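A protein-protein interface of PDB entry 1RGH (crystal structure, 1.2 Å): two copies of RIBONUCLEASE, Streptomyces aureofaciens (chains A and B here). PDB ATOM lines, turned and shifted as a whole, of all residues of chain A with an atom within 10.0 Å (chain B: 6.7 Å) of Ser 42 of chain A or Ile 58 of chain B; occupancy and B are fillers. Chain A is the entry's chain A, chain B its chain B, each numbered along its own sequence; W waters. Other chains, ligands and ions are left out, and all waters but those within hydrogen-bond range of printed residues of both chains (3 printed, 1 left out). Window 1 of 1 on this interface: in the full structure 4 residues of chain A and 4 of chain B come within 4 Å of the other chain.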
ATOM      1  N   ASP A   1       3.670 -28.090   1.582  1.00  0.00           N
ATOM      2  CA  ASP A   1       3.620 -28.657   2.904  1.00  0.00           C
ATOM      3  C   ASP A   1       3.494 -27.574   3.986  1.00  0.00           C
ATOM      4  O   ASP A   1       3.807 -26.410   3.767  1.00  0.00           O
ATOM      5  CB  ASP A   1       5.026 -29.357   3.165  1.00  0.00           C
ATOM      6  CG  ASP A   1       5.311 -30.229   1.926  1.00  0.00           C
ATOM      7  OD1 ASP A   1       4.388 -31.020   1.607  1.00  0.00           O
ATOM      8  OD2 ASP A   1       6.352 -30.022   1.289  1.00  0.00           O
ATOM      9  N   VAL A   2       3.122 -28.023   5.171  1.00  0.00           N
ATOM     10  CA  VAL A   2       2.985 -27.084   6.320  1.00  0.00           C
ATOM     11  C   VAL A   2       4.291 -27.139   7.089  1.00  0.00           C
ATOM     12  O   VAL A   2       4.830 -28.273   7.254  1.00  0.00           O
ATOM     13  CB  VAL A   2       1.842 -27.659   7.213  1.00  0.00           C
ATOM     14  CG1 VAL A   2       1.680 -26.738   8.418  1.00  0.00           C
ATOM     15  CG2 VAL A   2       0.538 -27.676   6.388  1.00  0.00           C
ATOM     16  N   PHE A  37      -9.946 -19.397  -0.249  1.00  0.00           N
ATOM     17  CA  PHE A  37      -8.542 -19.530  -0.576  1.00  0.00           C
ATOM     18  C   PHE A  37      -8.421 -20.750  -1.496  1.00  0.00           C
ATOM     19  O   PHE A  37      -8.758 -21.835  -1.097  1.00  0.00           O
ATOM     20  CB  PHE A  37      -7.687 -19.659   0.655  1.00  0.00           C
ATOM     21  CG  PHE A  37      -6.223 -19.867   0.381  1.00  0.00           C
ATOM     22  CD1 PHE A  37      -5.476 -18.809  -0.095  1.00  0.00           C
ATOM     23  CD2 PHE A  37      -5.610 -21.089   0.544  1.00  0.00           C
ATOM     24  CE1 PHE A  37      -4.110 -18.959  -0.317  1.00  0.00           C
ATOM     25  CE2 PHE A  37      -4.274 -21.255   0.278  1.00  0.00           C
ATOM     26  CZ  PHE A  37      -3.521 -20.182  -0.113  1.00  0.00           C
ATOM     27  N   GLN A  38      -7.951 -20.536  -2.726  1.00  0.00           N
ATOM     28  CA  GLN A  38      -7.935 -21.618  -3.709  1.00  0.00           C
ATOM     29  C   GLN A  38      -6.833 -22.623  -3.493  1.00  0.00           C
ATOM     30  O   GLN A  38      -6.918 -23.753  -4.073  1.00  0.00           O
ATOM     31  CB  GLN A  38      -7.651 -20.990  -5.102  1.00  0.00           C
ATOM     32  CG  GLN A  38      -8.794 -20.294  -5.769  1.00  0.00           C
ATOM     33  CD  GLN A  38      -8.427 -20.107  -7.273  1.00  0.00           C
ATOM     34  OE1 GLN A  38      -7.922 -21.040  -7.901  1.00  0.00           O
ATOM     35  NE2 GLN A  38      -8.582 -18.890  -7.691  1.00  0.00           N
ATOM     36  N   ASN A  39      -5.773 -22.314  -2.755  1.00  0.00           N
ATOM     37  CA  ASN A  39      -4.654 -23.247  -2.637  1.00  0.00           C
ATOM     38  C   ASN A  39      -4.141 -23.673  -4.017  1.00  0.00           C
ATOM     39  O   ASN A  39      -3.754 -24.842  -4.194  1.00  0.00           O
ATOM     40  CB  ASN A  39      -5.026 -24.481  -1.825  1.00  0.00           C
ATOM     41  CG  ASN A  39      -3.910 -25.305  -1.341  1.00  0.00           C
ATOM     42  OD1 ASN A  39      -2.824 -24.815  -1.047  1.00  0.00           O
ATOM     43  ND2 ASN A  39      -4.116 -26.645  -1.254  1.00  0.00           N
ATOM     44  N   ARG A  40      -4.001 -22.724  -4.905  1.00  0.00           N
ATOM     45  CA  ARG A  40      -3.602 -22.990  -6.296  1.00  0.00           C
ATOM     46  C   ARG A  40      -2.233 -23.579  -6.344  1.00  0.00           C
ATOM     47  O   ARG A  40      -1.973 -24.388  -7.298  1.00  0.00           O
ATOM     48  CB  ARG A  40      -3.694 -21.715  -7.119  1.00  0.00           C
ATOM     49  CG  ARG A  40      -3.440 -21.861  -8.592  1.00  0.00           C
ATOM     50  CD  ARG A  40      -3.605 -20.498  -9.310  1.00  0.00           C
ATOM     51  NE  ARG A  40      -2.881 -20.464 -10.550  1.00  0.00           N
ATOM     52  CZ  ARG A  40      -1.655 -20.135 -10.863  1.00  0.00           C
ATOM     53  NH1 ARG A  40      -0.910 -19.327 -10.121  1.00  0.00           N
ATOM     54  NH2 ARG A  40      -1.111 -20.563 -12.045  1.00  0.00           N
ATOM     55  N   GLU A  41      -1.316 -23.231  -5.460  1.00  0.00           N
ATOM     56  CA  GLU A  41       0.035 -23.756  -5.529  1.00  0.00           C
ATOM     57  C   GLU A  41       0.227 -25.038  -4.782  1.00  0.00           C
ATOM     58  O   GLU A  41       1.359 -25.543  -4.666  1.00  0.00           O
ATOM     59  CB  GLU A  41       1.055 -22.691  -5.087  1.00  0.00           C
ATOM     60  CG  GLU A  41       1.135 -21.463  -5.930  1.00  0.00           C
ATOM     61  CD  GLU A  41      -0.042 -20.532  -5.986  1.00  0.00           C
ATOM     62  OE1 GLU A  41      -0.732 -20.283  -4.967  1.00  0.00           O
ATOM     63  OE2 GLU A  41      -0.330 -20.031  -7.099  1.00  0.00           O
ATOM     64  N   SER A  42      -0.812 -25.598  -4.204  1.00  0.00           N
ATOM     65  CA  SER A  42      -0.759 -26.839  -3.486  1.00  0.00           C
ATOM     66  C   SER A  42       0.213 -26.887  -2.362  1.00  0.00           C
ATOM     67  O   SER A  42       0.760 -27.914  -1.994  1.00  0.00           O
ATOM     68  CB  SER A  42      -0.521 -27.985  -4.503  1.00  0.00           C
ATOM     69  OG  SER A  42      -0.831 -29.220  -3.924  1.00  0.00           O
ATOM     70  N   VAL A  43       0.326 -25.760  -1.620  1.00  0.00           N
ATOM     71  CA  VAL A  43       1.148 -25.726  -0.425  1.00  0.00           C
ATOM     72  C   VAL A  43       0.462 -26.398   0.747  1.00  0.00           C
ATOM     73  O   VAL A  43       1.026 -27.169   1.487  1.00  0.00           O
ATOM     74  CB  VAL A  43       1.590 -24.320  -0.084  1.00  0.00           C
ATOM     75  CG1 VAL A  43       2.561 -24.352   1.106  1.00  0.00           C
ATOM     76  CG2 VAL A  43       2.359 -23.694  -1.278  1.00  0.00           C
ATOM     77  N   LEU A  44      -0.880 -26.217   0.851  1.00  0.00           N
ATOM     78  CA  LEU A  44      -1.662 -26.890   1.863  1.00  0.00           C
ATOM     79  C   LEU A  44      -2.175 -28.231   1.333  1.00  0.00           C
ATOM     80  O   LEU A  44      -2.209 -28.385   0.071  1.00  0.00           O
ATOM     81  CB  LEU A  44      -2.842 -25.991   2.260  1.00  0.00           C
ATOM     82  CG  LEU A  44      -2.420 -24.674   2.986  1.00  0.00           C
ATOM     83  CD1 LEU A  44      -3.645 -23.866   3.343  1.00  0.00           C
ATOM     84  CD2 LEU A  44      -1.574 -24.931   4.173  1.00  0.00           C
ATOM     85  N   PRO A  45      -2.659 -29.095   2.156  1.00  0.00           N
ATOM     86  CA  PRO A  45      -3.267 -30.360   1.653  1.00  0.00           C
ATOM     87  C   PRO A  45      -4.330 -30.151   0.688  1.00  0.00           C
ATOM     88  O   PRO A  45      -5.185 -29.244   0.721  1.00  0.00           O
ATOM     89  CB  PRO A  45      -3.761 -31.064   2.950  1.00  0.00           C
ATOM     90  CG  PRO A  45      -2.872 -30.509   3.985  1.00  0.00           C
ATOM     91  CD  PRO A  45      -2.637 -29.077   3.643  1.00  0.00           C
ATOM     92  N   THR A  46      -4.380 -31.019  -0.369  1.00  0.00           N
ATOM     93  CA  THR A  46      -5.403 -30.933  -1.373  1.00  0.00           C
ATOM     94  C   THR A  46      -6.800 -31.185  -0.785  1.00  0.00           C
ATOM     95  O   THR A  46      -6.999 -32.172  -0.134  1.00  0.00           O
ATOM     96  CB  THR A  46      -5.145 -32.119  -2.388  1.00  0.00           C
ATOM     97  OG1 THR A  46      -3.868 -31.849  -3.013  1.00  0.00           O
ATOM     98  CG2 THR A  46      -6.177 -32.126  -3.469  1.00  0.00           C
ATOM     99  N   GLN A  47      -7.701 -30.266  -1.089  1.00  0.00           N
ATOM    100  CA  GLN A  47      -9.102 -30.373  -0.662  1.00  0.00           C
ATOM    101  C   GLN A  47      -9.995 -29.788  -1.717  1.00  0.00           C
ATOM    102  O   GLN A  47      -9.536 -29.088  -2.618  1.00  0.00           O
ATOM    103  CB  GLN A  47      -9.262 -29.641   0.679  1.00  0.00           C
ATOM    104  CG  GLN A  47      -8.541 -30.139   1.829  1.00  0.00           C
ATOM    105  CD  GLN A  47      -8.946 -31.431   2.482  1.00  0.00           C
ATOM    106  OE1 GLN A  47      -9.897 -32.103   1.965  1.00  0.00           O
ATOM    107  NE2 GLN A  47      -8.333 -31.824   3.558  1.00  0.00           N
ATOM    108  N   TYR A  52     -11.015 -24.100   2.183  1.00  0.00           N
ATOM    109  CA  TYR A  52     -10.185 -23.087   2.776  1.00  0.00           C
ATOM    110  C   TYR A  52     -10.760 -21.686   2.569  1.00  0.00           C
ATOM    111  O   TYR A  52     -11.204 -21.316   1.493  1.00  0.00           O
ATOM    112  CB  TYR A  52      -8.788 -23.132   2.213  1.00  0.00           C
ATOM    113  CG  TYR A  52      -8.034 -24.438   2.419  1.00  0.00           C
ATOM    114  CD1 TYR A  52      -7.570 -24.842   3.637  1.00  0.00           C
ATOM    115  CD2 TYR A  52      -7.704 -25.244   1.328  1.00  0.00           C
ATOM    116  CE1 TYR A  52      -6.818 -25.982   3.846  1.00  0.00           C
ATOM    117  CE2 TYR A  52      -6.973 -26.419   1.503  1.00  0.00           C
ATOM    118  CZ  TYR A  52      -6.544 -26.788   2.707  1.00  0.00           C
ATOM    119  OH  TYR A  52      -5.815 -27.926   2.925  1.00  0.00           O
ATOM    120  N   TYR A  86       1.478 -16.246   1.813  1.00  0.00           N
ATOM    121  CA  TYR A  86       1.111 -17.541   1.268  1.00  0.00           C
ATOM    122  C   TYR A  86       2.281 -18.393   0.889  1.00  0.00           C
ATOM    123  O   TYR A  86       2.071 -19.480   0.303  1.00  0.00           O
ATOM    124  CB  TYR A  86       0.024 -17.520   0.254  1.00  0.00           C
ATOM    125  CG  TYR A  86      -1.136 -16.567   0.429  1.00  0.00           C
ATOM    126  CD1 TYR A  86      -2.110 -16.770   1.375  1.00  0.00           C
ATOM    127  CD2 TYR A  86      -1.271 -15.466  -0.420  1.00  0.00           C
ATOM    128  CE1 TYR A  86      -3.183 -15.882   1.495  1.00  0.00           C
ATOM    129  CE2 TYR A  86      -2.301 -14.569  -0.271  1.00  0.00           C
ATOM    130  CZ  TYR A  86      -3.265 -14.800   0.692  1.00  0.00           C
ATOM    131  OH  TYR A  86      -4.319 -13.901   0.850  1.00  0.00           O
ATOM    132  N   ALA A  87       3.513 -17.967   1.202  1.00  0.00           N
ATOM    133  CA  ALA A  87       4.677 -18.740   0.835  1.00  0.00           C
ATOM    134  C   ALA A  87       4.864 -19.937   1.739  1.00  0.00           C
ATOM    135  O   ALA A  87       5.126 -21.054   1.245  1.00  0.00           O
ATOM    136  CB  ALA A  87       5.960 -17.914   0.844  1.00  0.00           C
ATOM    137  N   PHE A  89       3.467 -21.736   5.675  1.00  0.00           N
ATOM    138  CA  PHE A  89       2.364 -21.831   6.613  1.00  0.00           C
ATOM    139  C   PHE A  89       2.765 -22.636   7.810  1.00  0.00           C
ATOM    140  O   PHE A  89       3.451 -23.634   7.684  1.00  0.00           O
ATOM    141  CB  PHE A  89       1.166 -22.468   5.962  1.00  0.00           C
ATOM    142  CG  PHE A  89       0.505 -21.759   4.839  1.00  0.00           C
ATOM    143  CD1 PHE A  89       0.938 -21.955   3.518  1.00  0.00           C
ATOM    144  CD2 PHE A  89      -0.567 -20.916   5.038  1.00  0.00           C
ATOM    145  CE1 PHE A  89       0.381 -21.272   2.477  1.00  0.00           C
ATOM    146  CE2 PHE A  89      -1.182 -20.283   3.984  1.00  0.00           C
ATOM    147  CZ  PHE A  89      -0.777 -20.556   2.677  1.00  0.00           C
ATOM    148  N   PRO B  12       9.977 -33.281 -11.526  1.00  0.00           N
ATOM    149  CA  PRO B  12       9.457 -32.266 -10.610  1.00  0.00           C
ATOM    150  C   PRO B  12       9.474 -32.769  -9.207  1.00  0.00           C
ATOM    151  O   PRO B  12       9.374 -34.020  -8.962  1.00  0.00           O
ATOM    152  CB  PRO B  12       7.999 -32.090 -11.125  1.00  0.00           C
ATOM    153  CG  PRO B  12       8.081 -32.475 -12.566  1.00  0.00           C
ATOM    154  CD  PRO B  12       9.054 -33.637 -12.607  1.00  0.00           C
ATOM    155  N   GLU B  14       7.357 -32.952  -6.880  1.00  0.00           N
ATOM    156  CA  GLU B  14       6.128 -33.662  -6.455  1.00  0.00           C
ATOM    157  C   GLU B  14       6.225 -35.120  -6.848  1.00  0.00           C
ATOM    158  O   GLU B  14       5.493 -35.958  -6.259  1.00  0.00           O
ATOM    159  CB  GLU B  14       4.911 -32.993  -7.054  1.00  0.00           C
ATOM    160  CG  GLU B  14       4.679 -31.552  -6.614  1.00  0.00           C
ATOM    161  CD  GLU B  14       5.586 -30.540  -7.278  1.00  0.00           C
ATOM    162  OE1 GLU B  14       6.138 -30.737  -8.352  1.00  0.00           O
ATOM    163  OE2 GLU B  14       5.722 -29.429  -6.623  1.00  0.00           O
ATOM    164  N   ALA B  15       7.077 -35.516  -7.787  1.00  0.00           N
ATOM    165  CA  ALA B  15       7.228 -36.962  -8.083  1.00  0.00           C
ATOM    166  C   ALA B  15       7.802 -37.695  -6.915  1.00  0.00           C
ATOM    167  O   ALA B  15       7.446 -38.838  -6.599  1.00  0.00           O
ATOM    168  CB  ALA B  15       8.098 -37.142  -9.311  1.00  0.00           C
ATOM    169  N   ASP B  17       7.292 -36.755  -3.704  1.00  0.00           N
ATOM    170  CA  ASP B  17       6.198 -36.845  -2.798  1.00  0.00           C
ATOM    171  C   ASP B  17       5.312 -38.054  -3.097  1.00  0.00           C
ATOM    172  O   ASP B  17       4.934 -38.790  -2.209  1.00  0.00           O
ATOM    173  CB  ASP B  17       5.292 -35.610  -2.795  1.00  0.00           C
ATOM    174  CG  ASP B  17       6.045 -34.333  -2.479  1.00  0.00           C
ATOM    175  OD1 ASP B  17       7.080 -34.473  -1.793  1.00  0.00           O
ATOM    176  OD2 ASP B  17       5.518 -33.247  -2.832  1.00  0.00           O
ATOM    177  N   THR B  18       4.962 -38.236  -4.368  1.00  0.00           N
ATOM    178  CA  THR B  18       4.137 -39.385  -4.737  1.00  0.00           C
ATOM    179  C   THR B  18       4.841 -40.696  -4.441  1.00  0.00           C
ATOM    180  O   THR B  18       4.200 -41.625  -3.924  1.00  0.00           O
ATOM    181  CB  THR B  18       3.749 -39.306  -6.244  1.00  0.00           C
ATOM    182  OG1 THR B  18       3.073 -38.045  -6.402  1.00  0.00           O
ATOM    183  CG2 THR B  18       2.841 -40.434  -6.629  1.00  0.00           C
ATOM    184  N   PRO B  29      -3.964 -38.205  -1.687  1.00  0.00           N
ATOM    185  CA  PRO B  29      -4.812 -37.021  -1.825  1.00  0.00           C
ATOM    186  C   PRO B  29      -6.054 -37.206  -2.636  1.00  0.00           C
ATOM    187  O   PRO B  29      -7.074 -36.540  -2.316  1.00  0.00           O
ATOM    188  CB  PRO B  29      -3.911 -35.973  -2.472  1.00  0.00           C
ATOM    189  CG  PRO B  29      -2.914 -36.794  -3.254  1.00  0.00           C
ATOM    190  CD  PRO B  29      -2.677 -37.981  -2.347  1.00  0.00           C
ATOM    191  N   TYR B  30      -6.049 -38.015  -3.688  1.00  0.00           N
ATOM    192  CA  TYR B  30      -7.194 -38.168  -4.585  1.00  0.00           C
ATOM    193  C   TYR B  30      -7.815 -39.513  -4.462  1.00  0.00           C
ATOM    194  O   TYR B  30      -7.075 -40.531  -4.309  1.00  0.00           O
ATOM    195  CB  TYR B  30      -6.734 -37.922  -6.031  1.00  0.00           C
ATOM    196  CG  TYR B  30      -6.445 -36.452  -6.293  1.00  0.00           C
ATOM    197  CD1 TYR B  30      -7.526 -35.590  -6.500  1.00  0.00           C
ATOM    198  CD2 TYR B  30      -5.181 -35.947  -6.388  1.00  0.00           C
ATOM    199  CE1 TYR B  30      -7.348 -34.256  -6.750  1.00  0.00           C
ATOM    200  CE2 TYR B  30      -4.986 -34.585  -6.660  1.00  0.00           C
ATOM    201  CZ  TYR B  30      -6.069 -33.771  -6.819  1.00  0.00           C
ATOM    202  OH  TYR B  30      -5.856 -32.433  -7.152  1.00  0.00           O
ATOM    203  N   THR B  56      -1.411 -40.009  -8.769  1.00  0.00           N
ATOM    204  CA  THR B  56      -1.236 -38.623  -9.214  1.00  0.00           C
ATOM    205  C   THR B  56       0.090 -38.055  -8.741  1.00  0.00           C
ATOM    206  O   THR B  56       0.468 -38.218  -7.589  1.00  0.00           O
ATOM    207  CB  THR B  56      -2.355 -37.730  -8.565  1.00  0.00           C
ATOM    208  OG1 THR B  56      -3.643 -38.293  -8.822  1.00  0.00           O
ATOM    209  CG2 THR B  56      -2.349 -36.361  -9.198  1.00  0.00           C
ATOM    210  N   VAL B  57       0.718 -37.320  -9.646  1.00  0.00           N
ATOM    211  CA  VAL B  57       1.828 -36.426  -9.299  1.00  0.00           C
ATOM    212  C   VAL B  57       1.181 -35.016  -9.437  1.00  0.00           C
ATOM    213  O   VAL B  57       0.790 -34.606 -10.469  1.00  0.00           O
ATOM    214  CB  VAL B  57       3.025 -36.537 -10.231  1.00  0.00           C
ATOM    215  CG1 VAL B  57       4.029 -35.463  -9.947  1.00  0.00           C
ATOM    216  CG2 VAL B  57       3.644 -37.944 -10.109  1.00  0.00           C
ATOM    217  N   ILE B  58       1.070 -34.355  -8.276  1.00  0.00           N
ATOM    218  CA  ILE B  58       0.384 -33.042  -8.310  1.00  0.00           C
ATOM    219  C   ILE B  58       1.129 -32.058  -9.174  1.00  0.00           C
ATOM    220  O   ILE B  58       2.384 -32.004  -9.096  1.00  0.00           O
ATOM    221  CB  ILE B  58       0.292 -32.503  -6.845  1.00  0.00           C
ATOM    222  CG1 ILE B  58      -0.824 -33.352  -6.145  1.00  0.00           C
ATOM    223  CG2 ILE B  58      -0.122 -31.034  -6.845  1.00  0.00           C
ATOM    224  CD1 ILE B  58      -0.915 -33.069  -4.681  1.00  0.00           C
ATOM    225  N   THR B  59       0.452 -31.275  -9.946  1.00  0.00           N
ATOM    226  CA  THR B  59       1.026 -30.174 -10.713  1.00  0.00           C
ATOM    227  C   THR B  59       0.600 -28.853 -10.054  1.00  0.00           C
ATOM    228  O   THR B  59      -0.551 -28.470 -10.128  1.00  0.00           O
ATOM    229  CB  THR B  59       0.550 -30.162 -12.131  1.00  0.00           C
ATOM    230  OG1 THR B  59       0.944 -31.403 -12.780  1.00  0.00           O
ATOM    231  CG2 THR B  59       1.219 -29.066 -12.923  1.00  0.00           C
ATOM    232  N   PRO B  60       1.520 -28.161  -9.368  1.00  0.00           N
ATOM    233  CA  PRO B  60       1.107 -26.884  -8.743  1.00  0.00           C
ATOM    234  C   PRO B  60       0.664 -25.943  -9.802  1.00  0.00           C
ATOM    235  O   PRO B  60       1.216 -25.860 -10.895  1.00  0.00           O
ATOM    236  CB  PRO B  60       2.389 -26.385  -8.081  1.00  0.00           C
ATOM    237  CG  PRO B  60       3.342 -27.492  -8.076  1.00  0.00           C
ATOM    238  CD  PRO B  60       2.929 -28.495  -9.103  1.00  0.00           C
ATOM    239  N   GLY B  61      -0.398 -25.170  -9.556  1.00  0.00           N
ATOM    240  CA  GLY B  61      -0.932 -24.235 -10.456  1.00  0.00           C
ATOM    241  C   GLY B  61      -2.019 -24.751 -11.358  1.00  0.00           C
ATOM    242  O   GLY B  61      -2.775 -23.996 -11.958  1.00  0.00           O
ATOM    243  N   ALA B  62      -2.162 -26.089 -11.475  1.00  0.00           N
ATOM    244  CA  ALA B  62      -3.186 -26.665 -12.349  1.00  0.00           C
ATOM    245  C   ALA B  62      -4.530 -26.672 -11.660  1.00  0.00           C
ATOM    246  O   ALA B  62      -4.604 -26.829 -10.438  1.00  0.00           O
ATOM    247  CB  ALA B  62      -2.788 -28.096 -12.722  1.00  0.00           C
ATOM    248  N   ARG B  65      -6.412 -32.475 -11.755  1.00  0.00           N
ATOM    249  CA  ARG B  65      -5.382 -33.416 -11.384  1.00  0.00           C
ATOM    250  C   ARG B  65      -4.242 -33.356 -12.394  1.00  0.00           C
ATOM    251  O   ARG B  65      -3.164 -33.944 -12.098  1.00  0.00           O
ATOM    252  CB  ARG B  65      -5.894 -34.844 -11.307  1.00  0.00           C
ATOM    253  CG  ARG B  65      -6.623 -35.242 -10.085  1.00  0.00           C
ATOM    254  CD  ARG B  65      -6.789 -36.742  -9.938  1.00  0.00           C
ATOM    255  NE  ARG B  65      -7.054 -37.539 -11.077  1.00  0.00           N
ATOM    256  CZ  ARG B  65      -6.653 -38.760 -11.355  1.00  0.00           C
ATOM    257  NH1 ARG B  65      -5.562 -39.291 -10.817  1.00  0.00           N
ATOM    258  NH2 ARG B  65      -7.326 -39.472 -12.248  1.00  0.00           N
ATOM    259  N   ARG B  68       0.370 -35.476 -14.976  1.00  0.00           N
ATOM    260  CA  ARG B  68       1.514 -36.184 -14.434  1.00  0.00           C
ATOM    261  C   ARG B  68       1.102 -37.302 -13.549  1.00  0.00           C
ATOM    262  O   ARG B  68       0.272 -37.131 -12.649  1.00  0.00           O
ATOM    263  CB  ARG B  68       2.442 -35.184 -13.738  1.00  0.00           C
ATOM    264  CG  ARG B  68       2.854 -34.020 -14.537  1.00  0.00           C
ATOM    265  CD  ARG B  68       3.696 -32.987 -13.762  1.00  0.00           C
ATOM    266  NE  ARG B  68       4.061 -31.929 -14.731  1.00  0.00           N
ATOM    267  CZ  ARG B  68       4.833 -30.886 -14.408  1.00  0.00           C
ATOM    268  NH1 ARG B  68       5.174 -30.678 -13.209  1.00  0.00           N
ATOM    269  NH2 ARG B  68       5.170 -30.081 -15.406  1.00  0.00           N
ATOM    270  N   ARG B  69       1.731 -38.463 -13.739  1.00  0.00           N
ATOM    271  CA  ARG B  69       1.379 -39.655 -12.992  1.00  0.00           C
ATOM    272  C   ARG B  69       2.605 -40.545 -12.769  1.00  0.00           C
ATOM    273  O   ARG B  69       3.514 -40.479 -13.604  1.00  0.00           O
ATOM    274  CB  ARG B  69       0.366 -40.531 -13.763  1.00  0.00           C
ATOM    275  CG  ARG B  69      -0.889 -39.848 -14.211  1.00  0.00           C
ATOM    276  CD  ARG B  69      -1.909 -39.655 -13.137  1.00  0.00           C
ATOM    277  NE  ARG B  69      -3.153 -39.013 -13.561  1.00  0.00           N
ATOM    278  CZ  ARG B  69      -3.357 -37.722 -13.616  1.00  0.00           C
ATOM    279  NH1 ARG B  69      -2.511 -36.854 -13.177  1.00  0.00           N
ATOM    280  NH2 ARG B  69      -4.554 -37.270 -14.098  1.00  0.00           N
HETATM  281  O   HOH W   1      -5.242 -22.342 -11.316  1.00  0.00           O
HETATM  282  O   HOH W   2       4.994 -30.907  -1.786  1.00  0.00           O
HETATM  283  O   HOH W   3      -6.683 -34.946   0.008  1.00  0.00           O
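The backbone carbonyl oxygen (O) of Arg 40 of chain A sits at hydrogen-bond distance from the backbone NH (N) of Gly 61 of chain B.
OE2 of Glu 41 of chain A is in salt-bridge range of NH1 of Arg 40 of chain A, 3.2 Å away.
O of Arg 40 of chain A touches C of Pro 60 of chain B, at 3.95 Å. O of Glu 41 of chain A touches CB of Pro 60 of chain B (3.7 Å). Ser 42 of chain A touches Ile 58 of chain B (OG to CG2, 3.5 Å). CG2 of Thr 46 of chain A touches OH of Tyr 30 of chain B (3.7 Å). Thr 46 of chain A touches Ile 58 of chain B (OG1 to CD1, 3.6 Å).
Of the printed residues of chain B, Arg 40 of chain A touches Pro 60 (3.95 Å) and Gly 61 (2.9 Å). Of the printed residues of chain B, Glu 41 of chain A touches Pro 60. Of the printed residues of chain B, Ser 42 of chain A touches Ile 58. Printed residues of chain B within 4 Å of Thr 46 of chain A: Tyr 30 (3.7 Å) and Ile 58 (3.6 Å). Pro 12 of chain B touches none of the printed residues of chain A. No residue of chain A comes within 4 Å of Glu 14 of chain B. No residue of chain A comes within 4 Å of Val 57 of chain B. Printed residues of chain A within 4 Å of Ile 58 of chain B: Ser 42 (3.5 Å) and Thr 46 (3.6 Å). No residue of chain A comes within 4 Å of Thr 59 of chain B. Of the printed residues of chain A, Pro 60 of chain B touches Arg 40 and Glu 41. Printed residues of chain A within 4 Å of Gly 61 of chain B: Arg 40. The nearest printed residue of chain B that does not touch Ser 42 of chain A is Pro 60 of chain B (4.7 Å). The nearest printed residue of chain A that does not touch Ile 58 of chain B is Glu 41 of chain A (6.1 Å). The nearest printed residue of chain B that does not touch Arg 40 of chain A is Ala 62 of chain B (4.5 Å).
Printed residues of chain B that touch a printed residue of chain A: Tyr 30, Ile 58, Pro 60 and Gly 61. Hydrophobic or aromatic side chains of chain B that line the printed part of chain A: Tyr 30, Ile 58 and Pro 60. Of the 17 printed residues of chain A, 4 touch a printed residue of chain B. Along chain A the printed residues that touch a printed residue of chain B span positions 40 to 46. Among the printed residues, 6 pairs touch across the chains. Among the printed residues, no Asp or Glu carboxylate lies within 4 Å of a Lys or Arg side-chain nitrogen of the other chain.
No position is printed for both chains. Of the 6 pairs that touch across the chains among the printed residues, none has its exchanged pair printed and touching as well.
Water W2 bridges the side-chain carboxylate (OD2) of Asp 17 of chain B (2.6 Å) and the side-chain carboxylate (OD1) of Asp 1 of chain A (3.4 Å). Water W3 bridges the backbone carbonyl oxygen of Thr 46 of chain A (2.8 Å) and the backbone carbonyl oxygen of Pro 29 of chain B (2.8 Å). Water W1 lies within hydrogen-bond range of O of Gly 61 of chain B and NE of Arg 40 of chain A.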
